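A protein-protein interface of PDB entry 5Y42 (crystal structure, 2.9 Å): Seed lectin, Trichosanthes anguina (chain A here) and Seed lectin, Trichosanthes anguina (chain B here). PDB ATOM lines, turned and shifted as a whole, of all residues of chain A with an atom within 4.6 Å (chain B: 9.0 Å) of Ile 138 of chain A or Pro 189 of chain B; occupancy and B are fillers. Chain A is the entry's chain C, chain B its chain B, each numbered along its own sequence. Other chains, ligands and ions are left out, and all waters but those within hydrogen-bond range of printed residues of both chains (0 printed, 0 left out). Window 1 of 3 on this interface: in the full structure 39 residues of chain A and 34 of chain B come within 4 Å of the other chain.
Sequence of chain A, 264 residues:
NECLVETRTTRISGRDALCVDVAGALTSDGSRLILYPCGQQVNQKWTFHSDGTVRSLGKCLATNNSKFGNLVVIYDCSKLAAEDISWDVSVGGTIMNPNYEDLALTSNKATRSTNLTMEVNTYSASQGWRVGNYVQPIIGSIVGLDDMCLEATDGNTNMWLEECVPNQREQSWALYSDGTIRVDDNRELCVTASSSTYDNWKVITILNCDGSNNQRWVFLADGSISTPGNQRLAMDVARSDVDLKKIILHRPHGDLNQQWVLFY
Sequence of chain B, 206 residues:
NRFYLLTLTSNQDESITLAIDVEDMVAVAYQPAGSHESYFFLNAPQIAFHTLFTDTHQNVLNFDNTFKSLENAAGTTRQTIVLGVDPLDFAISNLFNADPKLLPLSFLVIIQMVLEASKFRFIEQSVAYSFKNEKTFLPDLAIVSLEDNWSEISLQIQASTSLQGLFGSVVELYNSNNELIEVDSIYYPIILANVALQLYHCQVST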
ATOM      1  N   ARG A 130      33.111 -10.559   0.588  1.00  0.00           N
ATOM      2  CA  ARG A 130      33.302 -11.831   1.273  1.00  0.00           C
ATOM      3  C   ARG A 130      34.755 -12.309   1.034  1.00  0.00           C
ATOM      4  O   ARG A 130      35.207 -12.611  -0.087  1.00  0.00           O
ATOM      5  CB  ARG A 130      32.399 -12.902   0.654  1.00  0.00           C
ATOM      6  CG  ARG A 130      32.413 -14.229   1.393  1.00  0.00           C
ATOM      7  CD  ARG A 130      31.892 -15.353   0.525  1.00  0.00           C
ATOM      8  NE  ARG A 130      30.461 -15.215   0.267  1.00  0.00           N
ATOM      9  CZ  ARG A 130      29.757 -15.949  -0.590  1.00  0.00           C
ATOM     10  NH1 ARG A 130      30.326 -16.918  -1.304  1.00  0.00           N
ATOM     11  NH2 ARG A 130      28.465 -15.713  -0.738  1.00  0.00           N
ATOM     12  N   TYR A 134      35.252 -19.901  -1.382  1.00  0.00           N
ATOM     13  CA  TYR A 134      33.999 -20.193  -2.047  1.00  0.00           C
ATOM     14  C   TYR A 134      33.325 -18.850  -2.332  1.00  0.00           C
ATOM     15  O   TYR A 134      32.879 -18.141  -1.452  1.00  0.00           O
ATOM     16  CB  TYR A 134      33.133 -21.070  -1.148  1.00  0.00           C
ATOM     17  CG  TYR A 134      31.900 -21.642  -1.787  1.00  0.00           C
ATOM     18  CD1 TYR A 134      31.938 -22.883  -2.408  1.00  0.00           C
ATOM     19  CD2 TYR A 134      30.682 -20.972  -1.734  1.00  0.00           C
ATOM     20  CE1 TYR A 134      30.814 -23.423  -2.995  1.00  0.00           C
ATOM     21  CE2 TYR A 134      29.548 -21.514  -2.319  1.00  0.00           C
ATOM     22  CZ  TYR A 134      29.633 -22.736  -2.935  1.00  0.00           C
ATOM     23  OH  TYR A 134      28.547 -23.282  -3.512  1.00  0.00           O
ATOM     24  N   GLN A 136      30.788 -18.354  -4.770  1.00  0.00           N
ATOM     25  CA  GLN A 136      29.429 -18.490  -5.309  1.00  0.00           C
ATOM     26  C   GLN A 136      28.386 -18.008  -4.333  1.00  0.00           C
ATOM     27  O   GLN A 136      28.540 -18.144  -3.125  1.00  0.00           O
ATOM     28  CB  GLN A 136      29.177 -19.974  -5.667  1.00  0.00           C
ATOM     29  CG  GLN A 136      30.190 -20.522  -6.680  1.00  0.00           C
ATOM     30  CD  GLN A 136      29.946 -21.961  -7.085  1.00  0.00           C
ATOM     31  OE1 GLN A 136      28.842 -22.338  -7.432  1.00  0.00           O
ATOM     32  NE2 GLN A 136      30.995 -22.759  -7.082  1.00  0.00           N
ATOM     33  N   PRO A 137      27.259 -17.469  -4.825  1.00  0.00           N
ATOM     34  CA  PRO A 137      26.033 -17.265  -4.080  1.00  0.00           C
ATOM     35  C   PRO A 137      25.553 -18.490  -3.285  1.00  0.00           C
ATOM     36  O   PRO A 137      25.722 -19.621  -3.811  1.00  0.00           O
ATOM     37  CB  PRO A 137      25.020 -16.984  -5.187  1.00  0.00           C
ATOM     38  CG  PRO A 137      25.814 -16.315  -6.235  1.00  0.00           C
ATOM     39  CD  PRO A 137      27.171 -16.923  -6.188  1.00  0.00           C
ATOM     40  N   ILE A 138      25.100 -18.302  -2.072  1.00  0.00           N
ATOM     41  CA  ILE A 138      24.581 -19.394  -1.275  1.00  0.00           C
ATOM     42  C   ILE A 138      23.061 -19.367  -1.403  1.00  0.00           C
ATOM     43  O   ILE A 138      22.384 -18.402  -1.006  1.00  0.00           O
ATOM     44  CB  ILE A 138      25.023 -19.248   0.187  1.00  0.00           C
ATOM     45  CG1 ILE A 138      26.556 -19.222   0.247  1.00  0.00           C
ATOM     46  CG2 ILE A 138      24.487 -20.376   1.074  1.00  0.00           C
ATOM     47  CD1 ILE A 138      27.071 -18.469   1.443  1.00  0.00           C
ATOM     48  N   ILE A 139      22.522 -20.471  -1.950  1.00  0.00           N
ATOM     49  CA  ILE A 139      21.064 -20.495  -2.204  1.00  0.00           C
ATOM     50  C   ILE A 139      20.310 -21.305  -1.177  1.00  0.00           C
ATOM     51  O   ILE A 139      20.569 -22.472  -1.051  1.00  0.00           O
ATOM     52  CB  ILE A 139      20.733 -20.939  -3.641  1.00  0.00           C
ATOM     53  CG1 ILE A 139      21.308 -19.931  -4.655  1.00  0.00           C
ATOM     54  CG2 ILE A 139      19.204 -20.998  -3.864  1.00  0.00           C
ATOM     55  CD1 ILE A 139      22.810 -19.839  -4.697  1.00  0.00           C
ATOM     56  N   GLY A 140      19.293 -20.635  -0.587  1.00  0.00           N
ATOM     57  CA  GLY A 140      18.355 -21.344   0.286  1.00  0.00           C
ATOM     58  C   GLY A 140      17.060 -20.617   0.533  1.00  0.00           C
ATOM     59  O   GLY A 140      16.797 -19.557  -0.032  1.00  0.00           O
ATOM     60  N   TRP A 173      16.131 -17.930  -2.393  1.00  0.00           N
ATOM     61  CA  TRP A 173      16.942 -16.730  -2.363  1.00  0.00           C
ATOM     62  C   TRP A 173      18.426 -17.063  -2.563  1.00  0.00           C
ATOM     63  O   TRP A 173      18.918 -18.143  -2.199  1.00  0.00           O
ATOM     64  CB  TRP A 173      16.712 -16.018  -1.026  1.00  0.00           C
ATOM     65  CG  TRP A 173      15.274 -15.724  -0.771  1.00  0.00           C
ATOM     66  CD1 TRP A 173      14.373 -16.503  -0.098  1.00  0.00           C
ATOM     67  CD2 TRP A 173      14.566 -14.577  -1.214  1.00  0.00           C
ATOM     68  NE1 TRP A 173      13.146 -15.898  -0.087  1.00  0.00           N
ATOM     69  CE2 TRP A 173      13.229 -14.713  -0.768  1.00  0.00           C
ATOM     70  CE3 TRP A 173      14.933 -13.435  -1.945  1.00  0.00           C
ATOM     71  CZ2 TRP A 173      12.243 -13.745  -1.022  1.00  0.00           C
ATOM     72  CZ3 TRP A 173      13.957 -12.470  -2.209  1.00  0.00           C
ATOM     73  CH2 TRP A 173      12.617 -12.638  -1.746  1.00  0.00           C
ATOM     74  N   ALA A 174      19.132 -16.115  -3.138  1.00  0.00           N
ATOM     75  CA  ALA A 174      20.550 -16.274  -3.379  1.00  0.00           C
ATOM     76  C   ALA A 174      21.291 -15.173  -2.667  1.00  0.00           C
ATOM     77  O   ALA A 174      21.044 -13.998  -2.936  1.00  0.00           O
ATOM     78  CB  ALA A 174      20.901 -16.311  -4.855  1.00  0.00           C
ATOM     79  N   LEU A 175      22.167 -15.566  -1.725  1.00  0.00           N
ATOM     80  CA  LEU A 175      22.961 -14.644  -0.931  1.00  0.00           C
ATOM     81  C   LEU A 175      24.332 -14.415  -1.584  1.00  0.00           C
ATOM     82  O   LEU A 175      25.136 -15.335  -1.690  1.00  0.00           O
ATOM     83  CB  LEU A 175      23.189 -15.179   0.494  1.00  0.00           C
ATOM     84  CG  LEU A 175      22.054 -15.129   1.533  1.00  0.00           C
ATOM     85  CD1 LEU A 175      20.783 -15.751   0.993  1.00  0.00           C
ATOM     86  CD2 LEU A 175      22.436 -15.845   2.814  1.00  0.00           C
ATOM     87  N   PHE A 219      23.634 -11.669   7.812  1.00  0.00           N
ATOM     88  CA  PHE A 219      23.071 -12.658   8.726  1.00  0.00           C
ATOM     89  C   PHE A 219      23.983 -12.813   9.935  1.00  0.00           C
ATOM     90  O   PHE A 219      25.084 -13.319   9.807  1.00  0.00           O
ATOM     91  CB  PHE A 219      22.870 -14.015   8.107  1.00  0.00           C
ATOM     92  CG  PHE A 219      21.725 -14.113   7.149  1.00  0.00           C
ATOM     93  CD1 PHE A 219      21.749 -13.430   5.939  1.00  0.00           C
ATOM     94  CD2 PHE A 219      20.672 -14.989   7.394  1.00  0.00           C
ATOM     95  CE1 PHE A 219      20.725 -13.583   5.017  1.00  0.00           C
ATOM     96  CE2 PHE A 219      19.642 -15.138   6.472  1.00  0.00           C
ATOM     97  CZ  PHE A 219      19.668 -14.435   5.281  1.00  0.00           C
ATOM     98  N   LEU A 262      18.563 -19.456   7.818  1.00  0.00           N
ATOM     99  CA  LEU A 262      18.868 -19.750   6.432  1.00  0.00           C
ATOM    100  C   LEU A 262      18.763 -21.248   6.235  1.00  0.00           C
ATOM    101  O   LEU A 262      19.533 -21.987   6.840  1.00  0.00           O
ATOM    102  CB  LEU A 262      20.274 -19.269   6.104  1.00  0.00           C
ATOM    103  CG  LEU A 262      20.744 -19.538   4.684  1.00  0.00           C
ATOM    104  CD1 LEU A 262      20.006 -18.632   3.708  1.00  0.00           C
ATOM    105  CD2 LEU A 262      22.249 -19.339   4.581  1.00  0.00           C
ATOM    106  N   PHE B 120      23.360 -26.173  16.262  1.00  0.00           N
ATOM    107  CA  PHE B 120      23.122 -25.581  14.951  1.00  0.00           C
ATOM    108  C   PHE B 120      21.688 -25.186  14.654  1.00  0.00           C
ATOM    109  O   PHE B 120      20.767 -25.941  14.905  1.00  0.00           O
ATOM    110  CB  PHE B 120      23.539 -26.564  13.862  1.00  0.00           C
ATOM    111  CG  PHE B 120      24.987 -26.926  13.883  1.00  0.00           C
ATOM    112  CD1 PHE B 120      25.929 -26.057  13.403  1.00  0.00           C
ATOM    113  CD2 PHE B 120      25.398 -28.148  14.356  1.00  0.00           C
ATOM    114  CE1 PHE B 120      27.260 -26.386  13.410  1.00  0.00           C
ATOM    115  CE2 PHE B 120      26.727 -28.488  14.367  1.00  0.00           C
ATOM    116  CZ  PHE B 120      27.659 -27.603  13.893  1.00  0.00           C
ATOM    117  N   ARG B 121      21.507 -23.989  14.120  1.00  0.00           N
ATOM    118  CA  ARG B 121      20.187 -23.528  13.744  1.00  0.00           C
ATOM    119  C   ARG B 121      19.602 -24.356  12.613  1.00  0.00           C
ATOM    120  O   ARG B 121      18.414 -24.640  12.598  1.00  0.00           O
ATOM    121  CB  ARG B 121      20.202 -22.045  13.400  1.00  0.00           C
ATOM    122  CG  ARG B 121      20.325 -21.181  14.632  1.00  0.00           C
ATOM    123  CD  ARG B 121      20.045 -19.721  14.365  1.00  0.00           C
ATOM    124  NE  ARG B 121      20.211 -18.971  15.599  1.00  0.00           N
ATOM    125  CZ  ARG B 121      21.186 -18.103  15.825  1.00  0.00           C
ATOM    126  NH1 ARG B 121      22.079 -17.842  14.891  1.00  0.00           N
ATOM    127  NH2 ARG B 121      21.255 -17.486  16.988  1.00  0.00           N
ATOM    128  N   PHE B 122      20.434 -24.734  11.654  1.00  0.00           N
ATOM    129  CA  PHE B 122      19.945 -25.539  10.546  1.00  0.00           C
ATOM    130  C   PHE B 122      19.300 -26.850  10.999  1.00  0.00           C
ATOM    131  O   PHE B 122      18.293 -27.305  10.417  1.00  0.00           O
ATOM    132  CB  PHE B 122      21.061 -25.843   9.565  1.00  0.00           C
ATOM    133  CG  PHE B 122      20.595 -26.628   8.378  1.00  0.00           C
ATOM    134  CD1 PHE B 122      19.851 -26.017   7.390  1.00  0.00           C
ATOM    135  CD2 PHE B 122      20.851 -27.973   8.284  1.00  0.00           C
ATOM    136  CE1 PHE B 122      19.389 -26.724   6.296  1.00  0.00           C
ATOM    137  CE2 PHE B 122      20.412 -28.700   7.205  1.00  0.00           C
ATOM    138  CZ  PHE B 122      19.663 -28.074   6.205  1.00  0.00           C
ATOM    139  N   LEU B 146      27.583 -31.047   9.497  1.00  0.00           N
ATOM    140  CA  LEU B 146      27.577 -30.137  10.633  1.00  0.00           C
ATOM    141  C   LEU B 146      27.911 -30.900  11.918  1.00  0.00           C
ATOM    142  O   LEU B 146      28.754 -30.468  12.695  1.00  0.00           O
ATOM    143  CB  LEU B 146      26.246 -29.414  10.753  1.00  0.00           C
ATOM    144  CG  LEU B 146      25.938 -28.448   9.605  1.00  0.00           C
ATOM    145  CD1 LEU B 146      24.497 -28.022   9.779  1.00  0.00           C
ATOM    146  CD2 LEU B 146      26.863 -27.233   9.599  1.00  0.00           C
ATOM    147  N   LEU B 173      31.521 -28.679   4.194  1.00  0.00           N
ATOM    148  CA  LEU B 173      30.118 -28.812   4.552  1.00  0.00           C
ATOM    149  C   LEU B 173      29.273 -29.013   3.288  1.00  0.00           C
ATOM    150  O   LEU B 173      29.725 -28.734   2.162  1.00  0.00           O
ATOM    151  CB  LEU B 173      29.587 -27.580   5.298  1.00  0.00           C
ATOM    152  CG  LEU B 173      30.247 -27.256   6.626  1.00  0.00           C
ATOM    153  CD1 LEU B 173      29.798 -25.911   7.161  1.00  0.00           C
ATOM    154  CD2 LEU B 173      29.957 -28.326   7.640  1.00  0.00           C
ATOM    155  N   TYR B 174      28.049 -29.443   3.469  1.00  0.00           N
ATOM    156  CA  TYR B 174      27.195 -29.699   2.335  1.00  0.00           C
ATOM    157  C   TYR B 174      25.902 -28.939   2.453  1.00  0.00           C
ATOM    158  O   TYR B 174      25.471 -28.674   3.560  1.00  0.00           O
ATOM    159  CB  TYR B 174      26.989 -31.192   2.252  1.00  0.00           C
ATOM    160  CG  TYR B 174      28.250 -31.915   1.825  1.00  0.00           C
ATOM    161  CD1 TYR B 174      28.546 -32.107   0.480  1.00  0.00           C
ATOM    162  CD2 TYR B 174      29.153 -32.391   2.753  1.00  0.00           C
ATOM    163  CE1 TYR B 174      29.686 -32.786   0.088  1.00  0.00           C
ATOM    164  CE2 TYR B 174      30.302 -33.082   2.363  1.00  0.00           C
ATOM    165  CZ  TYR B 174      30.564 -33.273   1.028  1.00  0.00           C
ATOM    166  OH  TYR B 174      31.706 -33.941   0.636  1.00  0.00           O
ATOM    167  N   ASN B 175      25.317 -28.569   1.320  1.00  0.00           N
ATOM    168  CA  ASN B 175      23.964 -28.001   1.276  1.00  0.00           C
ATOM    169  C   ASN B 175      22.956 -29.104   1.077  1.00  0.00           C
ATOM    170  O   ASN B 175      23.303 -30.268   1.022  1.00  0.00           O
ATOM    171  CB  ASN B 175      23.899 -26.901   0.212  1.00  0.00           C
ATOM    172  CG  ASN B 175      23.802 -27.404  -1.224  1.00  0.00           C
ATOM    173  OD1 ASN B 175      23.594 -28.600  -1.542  1.00  0.00           O
ATOM    174  ND2 ASN B 175      23.942 -26.438  -2.127  1.00  0.00           N
ATOM    175  N   SER B 176      21.691 -28.700   0.965  1.00  0.00           N
ATOM    176  CA  SER B 176      20.546 -29.635   0.981  1.00  0.00           C
ATOM    177  C   SER B 176      20.490 -30.517  -0.277  1.00  0.00           C
ATOM    178  O   SER B 176      19.878 -31.586  -0.301  1.00  0.00           O
ATOM    179  CB  SER B 176      19.210 -28.873   1.186  1.00  0.00           C
ATOM    180  OG  SER B 176      19.115 -28.256   2.476  1.00  0.00           O
ATOM    181  N   GLU B 179      25.618 -30.600  -2.417  1.00  0.00           N
ATOM    182  CA  GLU B 179      26.726 -29.916  -3.055  1.00  0.00           C
ATOM    183  C   GLU B 179      27.729 -29.505  -2.003  1.00  0.00           C
ATOM    184  O   GLU B 179      27.332 -29.091  -0.953  1.00  0.00           O
ATOM    185  CB  GLU B 179      26.226 -28.680  -3.777  1.00  0.00           C
ATOM    186  CG  GLU B 179      25.106 -28.958  -4.760  1.00  0.00           C
ATOM    187  CD  GLU B 179      24.739 -27.706  -5.541  1.00  0.00           C
ATOM    188  OE1 GLU B 179      24.654 -26.606  -4.963  1.00  0.00           O
ATOM    189  OE2 GLU B 179      24.539 -27.818  -6.762  1.00  0.00           O
ATOM    190  N   ILE B 181      30.414 -27.313  -0.032  1.00  0.00           N
ATOM    191  CA  ILE B 181      30.787 -25.942   0.211  1.00  0.00           C
ATOM    192  C   ILE B 181      31.994 -25.947   1.128  1.00  0.00           C
ATOM    193  O   ILE B 181      31.874 -26.227   2.322  1.00  0.00           O
ATOM    194  CB  ILE B 181      29.619 -25.161   0.829  1.00  0.00           C
ATOM    195  CG1 ILE B 181      28.423 -25.144  -0.145  1.00  0.00           C
ATOM    196  CG2 ILE B 181      30.052 -23.752   1.203  1.00  0.00           C
ATOM    197  CD1 ILE B 181      27.180 -24.426   0.360  1.00  0.00           C
ATOM    198  N   GLU B 182      33.172 -25.647   0.570  1.00  0.00           N
ATOM    199  CA  GLU B 182      34.406 -25.582   1.341  1.00  0.00           C
ATOM    200  C   GLU B 182      34.505 -24.206   1.992  1.00  0.00           C
ATOM    201  O   GLU B 182      34.593 -23.191   1.308  1.00  0.00           O
ATOM    202  CB  GLU B 182      35.614 -25.783   0.409  1.00  0.00           C
ATOM    203  CG  GLU B 182      35.646 -27.148  -0.279  1.00  0.00           C
ATOM    204  CD  GLU B 182      37.021 -27.549  -0.823  1.00  0.00           C
ATOM    205  OE1 GLU B 182      37.925 -27.873  -0.032  1.00  0.00           O
ATOM    206  OE2 GLU B 182      37.205 -27.567  -2.057  1.00  0.00           O
ATOM    207  N   VAL B 183      34.482 -24.180   3.314  1.00  0.00           N
ATOM    208  CA  VAL B 183      34.463 -22.951   4.082  1.00  0.00           C
ATOM    209  C   VAL B 183      35.838 -22.748   4.724  1.00  0.00           C
ATOM    210  O   VAL B 183      36.380 -23.632   5.390  1.00  0.00           O
ATOM    211  CB  VAL B 183      33.395 -23.093   5.161  1.00  0.00           C
ATOM    212  CG1 VAL B 183      33.271 -21.821   5.958  1.00  0.00           C
ATOM    213  CG2 VAL B 183      32.062 -23.435   4.519  1.00  0.00           C
ATOM    214  N   SER B 185      36.581 -19.474   6.307  1.00  0.00           N
ATOM    215  CA  SER B 185      36.458 -18.171   6.969  1.00  0.00           C
ATOM    216  C   SER B 185      35.166 -18.094   7.723  1.00  0.00           C
ATOM    217  O   SER B 185      34.283 -18.869   7.491  1.00  0.00           O
ATOM    218  CB  SER B 185      36.527 -17.011   5.981  1.00  0.00           C
ATOM    219  OG  SER B 185      35.307 -16.824   5.316  1.00  0.00           O
ATOM    220  N   ILE B 186      35.038 -17.105   8.594  1.00  0.00           N
ATOM    221  CA  ILE B 186      33.785 -16.843   9.280  1.00  0.00           C
ATOM    222  C   ILE B 186      32.738 -16.118   8.408  1.00  0.00           C
ATOM    223  O   ILE B 186      31.586 -16.007   8.764  1.00  0.00           O
ATOM    224  CB  ILE B 186      34.079 -16.055  10.564  1.00  0.00           C
ATOM    225  CG1 ILE B 186      32.970 -16.222  11.587  1.00  0.00           C
ATOM    226  CG2 ILE B 186      34.233 -14.577  10.289  1.00  0.00           C
ATOM    227  CD1 ILE B 186      32.878 -17.618  12.149  1.00  0.00           C
ATOM    228  N   TYR B 187      33.107 -15.683   7.216  1.00  0.00           N
ATOM    229  CA  TYR B 187      32.270 -14.775   6.433  1.00  0.00           C
ATOM    230  C   TYR B 187      31.306 -15.604   5.563  1.00  0.00           C
ATOM    231  O   TYR B 187      31.123 -15.382   4.377  1.00  0.00           O
ATOM    232  CB  TYR B 187      33.138 -13.850   5.566  1.00  0.00           C
ATOM    233  CG  TYR B 187      34.144 -13.085   6.386  1.00  0.00           C
ATOM    234  CD1 TYR B 187      33.722 -12.136   7.329  1.00  0.00           C
ATOM    235  CD2 TYR B 187      35.508 -13.338   6.269  1.00  0.00           C
ATOM    236  CE1 TYR B 187      34.632 -11.457   8.109  1.00  0.00           C
ATOM    237  CE2 TYR B 187      36.432 -12.656   7.047  1.00  0.00           C
ATOM    238  CZ  TYR B 187      35.985 -11.718   7.963  1.00  0.00           C
ATOM    239  OH  TYR B 187      36.861 -11.023   8.746  1.00  0.00           O
ATOM    240  N   TYR B 188      30.732 -16.620   6.151  1.00  0.00           N
ATOM    241  CA  TYR B 188      29.691 -17.406   5.524  1.00  0.00           C
ATOM    242  C   TYR B 188      28.528 -17.557   6.514  1.00  0.00           C
ATOM    243  O   TYR B 188      28.768 -17.891   7.677  1.00  0.00           O
ATOM    244  CB  TYR B 188      30.219 -18.780   5.117  1.00  0.00           C
ATOM    245  CG  TYR B 188      31.243 -18.760   4.026  1.00  0.00           C
ATOM    246  CD1 TYR B 188      32.579 -18.625   4.318  1.00  0.00           C
ATOM    247  CD2 TYR B 188      30.881 -18.907   2.689  1.00  0.00           C
ATOM    248  CE1 TYR B 188      33.546 -18.617   3.310  1.00  0.00           C
ATOM    249  CE2 TYR B 188      31.833 -18.891   1.665  1.00  0.00           C
ATOM    250  CZ  TYR B 188      33.177 -18.740   1.986  1.00  0.00           C
ATOM    251  OH  TYR B 188      34.167 -18.724   1.030  1.00  0.00           O
ATOM    252  N   PRO B 189      27.289 -17.285   6.074  1.00  0.00           N
ATOM    253  CA  PRO B 189      26.200 -17.413   7.035  1.00  0.00           C
ATOM    254  C   PRO B 189      25.990 -18.826   7.537  1.00  0.00           C
ATOM    255  O   PRO B 189      25.366 -18.984   8.565  1.00  0.00           O
ATOM    256  CB  PRO B 189      24.966 -16.882   6.277  1.00  0.00           C
ATOM    257  CG  PRO B 189      25.291 -17.036   4.846  1.00  0.00           C
ATOM    258  CD  PRO B 189      26.796 -16.954   4.726  1.00  0.00           C
ATOM    259  N   ILE B 190      26.413 -19.815   6.741  1.00  0.00           N
ATOM    260  CA  ILE B 190      26.316 -21.216   7.169  1.00  0.00           C
ATOM    261  C   ILE B 190      27.229 -21.534   8.341  1.00  0.00           C
ATOM    262  O   ILE B 190      27.078 -22.624   8.925  1.00  0.00           O
ATOM    263  CB  ILE B 190      26.525 -22.256   6.030  1.00  0.00           C
ATOM    264  CG1 ILE B 190      27.976 -22.294   5.554  1.00  0.00           C
ATOM    265  CG2 ILE B 190      25.560 -21.980   4.886  1.00  0.00           C
ATOM    266  CD1 ILE B 190      28.203 -23.272   4.442  1.00  0.00           C
ATOM    267  N   ILE B 191      28.160 -20.629   8.679  1.00  0.00           N
ATOM    268  CA  ILE B 191      28.851 -20.731   9.922  1.00  0.00           C
ATOM    269  C   ILE B 191      28.343 -19.758  10.943  1.00  0.00           C
ATOM    270  O   ILE B 191      27.809 -20.105  11.947  1.00  0.00           O
ATOM    271  CB  ILE B 191      30.393 -20.549   9.795  1.00  0.00           C
ATOM    272  CG1 ILE B 191      30.998 -21.551   8.818  1.00  0.00           C
ATOM    273  CG2 ILE B 191      31.080 -20.694  11.144  1.00  0.00           C
ATOM    274  CD1 ILE B 191      30.682 -22.992   9.113  1.00  0.00           C
ATOM    275  N   LEU B 192      28.438 -18.479  10.635  1.00  0.00           N
ATOM    276  CA  LEU B 192      28.189 -17.430  11.601  1.00  0.00           C
ATOM    277  C   LEU B 192      26.745 -17.356  12.091  1.00  0.00           C
ATOM    278  O   LEU B 192      26.520 -17.091  13.273  1.00  0.00           O
ATOM    279  CB  LEU B 192      28.590 -16.075  11.064  1.00  0.00           C
ATOM    280  CG  LEU B 192      28.452 -14.836  11.959  1.00  0.00           C
ATOM    281  CD1 LEU B 192      29.522 -14.735  13.034  1.00  0.00           C
ATOM    282  CD2 LEU B 192      28.570 -13.647  11.060  1.00  0.00           C
ATOM    283  N   ALA B 193      25.775 -17.615  11.207  1.00  0.00           N
ATOM    284  CA  ALA B 193      24.368 -17.600  11.573  1.00  0.00           C
ATOM    285  C   ALA B 193      23.815 -18.980  11.969  1.00  0.00           C
ATOM    286  O   ALA B 193      22.661 -19.106  12.302  1.00  0.00           O
ATOM    287  CB  ALA B 193      23.544 -17.029  10.439  1.00  0.00           C
ATOM    288  N   ASN B 194      24.675 -19.977  11.903  1.00  0.00           N
ATOM    289  CA  ASN B 194      24.254 -21.368  12.078  1.00  0.00           C
ATOM    290  C   ASN B 194      24.666 -21.872  13.462  1.00  0.00           C
ATOM    291  O   ASN B 194      23.822 -22.343  14.253  1.00  0.00           O
ATOM    292  CB  ASN B 194      24.849 -22.198  10.934  1.00  0.00           C
ATOM    293  CG  ASN B 194      24.239 -23.568  10.822  1.00  0.00           C
ATOM    294  OD1 ASN B 194      23.227 -23.855  11.440  1.00  0.00           O
ATOM    295  ND2 ASN B 194      24.857 -24.426  10.030  1.00  0.00           N
ATOM    296  N   VAL B 195      25.950 -21.735  13.757  1.00  0.00           N
ATOM    297  CA  VAL B 195      26.559 -22.235  14.991  1.00  0.00           C
ATOM    298  C   VAL B 195      26.111 -21.430  16.211  1.00  0.00           C
ATOM    299  O   VAL B 195      26.501 -20.241  16.349  1.00  0.00           O
ATOM    300  CB  VAL B 195      28.096 -22.185  14.909  1.00  0.00           C
ATOM    301  CG1 VAL B 195      28.704 -22.705  16.197  1.00  0.00           C
ATOM    302  CG2 VAL B 195      28.603 -22.973  13.720  1.00  0.00           C
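Printed residues of chain A within 4 Å of Pro 189 of chain B: Ile 138 (3.6 Å), Leu 175 (3.7 Å), Phe 219 (3.995 Å) and Leu 262 (3.8 Å). No residue of chain B comes within 4 Å of Pro 137 of chain A. Ile 139 of chain A touches none of the printed residues of chain B. Printed residues of chain B within 4 Å of Leu 175 of chain A: Pro 189 (3.7 Å). Of the printed residues of chain B, Tyr 134 of chain A touches Ile 181 (3.8 Å), Glu 182 (3.6 Å) and Tyr 188 (2.9 Å). Printed residues of chain B within 4 Å of Phe 219 of chain A: Pro 189, Leu 192 and Ala 193. Of the printed residues of chain A, Ile 181 of chain B touches Tyr 134. Of the printed residues of chain B, Arg 130 of chain A touches Tyr 187 and Tyr 188.
Along chain A the printed residues that touch a printed residue of chain B span positions 130 to 262. Hydrophobic or aromatic side chains of chain B within 4 Å of the printed part of chain A: Ile 181, Tyr 188, Pro 189, Leu 192 and Ala 193. Among the printed residues, 11 pairs touch across the chains.
NH1 of Arg 130 of chain A sits at hydrogen-bond distance from O of Gln 136 of chain A, at 2.8 Å. O of Ala 193 of chain B sits at hydrogen-bond distance from NH1 of Arg 121 of chain B (2.9 Å). O of Leu 173 of chain B sits at hydrogen-bond distance from N of Ile 181 of chain B (2.7 Å). N of Leu 175 of chain A is in hydrogen-bond range of O of Ile 138 of chain A (2.9 Å). O of Leu 175 of chain A lies within hydrogen-bond range of NH2 of Arg 130 of chain A. NH1 of Arg 130 of chain A is in hydrogen-bond range of O of Tyr 134 of chain A, at 2.8 Å.
The side-chain hydroxyl (OH) of Tyr 188 of chain B sits at hydrogen-bond distance from the backbone carbonyl oxygen (O) of Tyr 134 of chain A (2.9 Å).
Tyr 187 of chain B touches Arg 130 of chain A. Arg 130 of chain A touches Tyr 188 of chain B. Tyr 134 of chain A touches Ile 181 of chain B. Tyr 134 of chain A touches Glu 182 of chain B (CB to O, 3.6 Å). CD1 of Ile 138 of chain A touches CD of Pro 189 of chain B, 3.6 Å away. Leu 175 of chain A touches Pro 189 of chain B. Pro 189 of chain B touches Phe 219 of chain A. O of Phe 219 of chain A touches CD2 of Leu 192 of chain B, 3.7 Å away. Phe 219 of chain A touches Ala 193 of chain B (CB to CB, 3.9 Å). Leu 262 of chain A touches Pro 189 of chain B.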
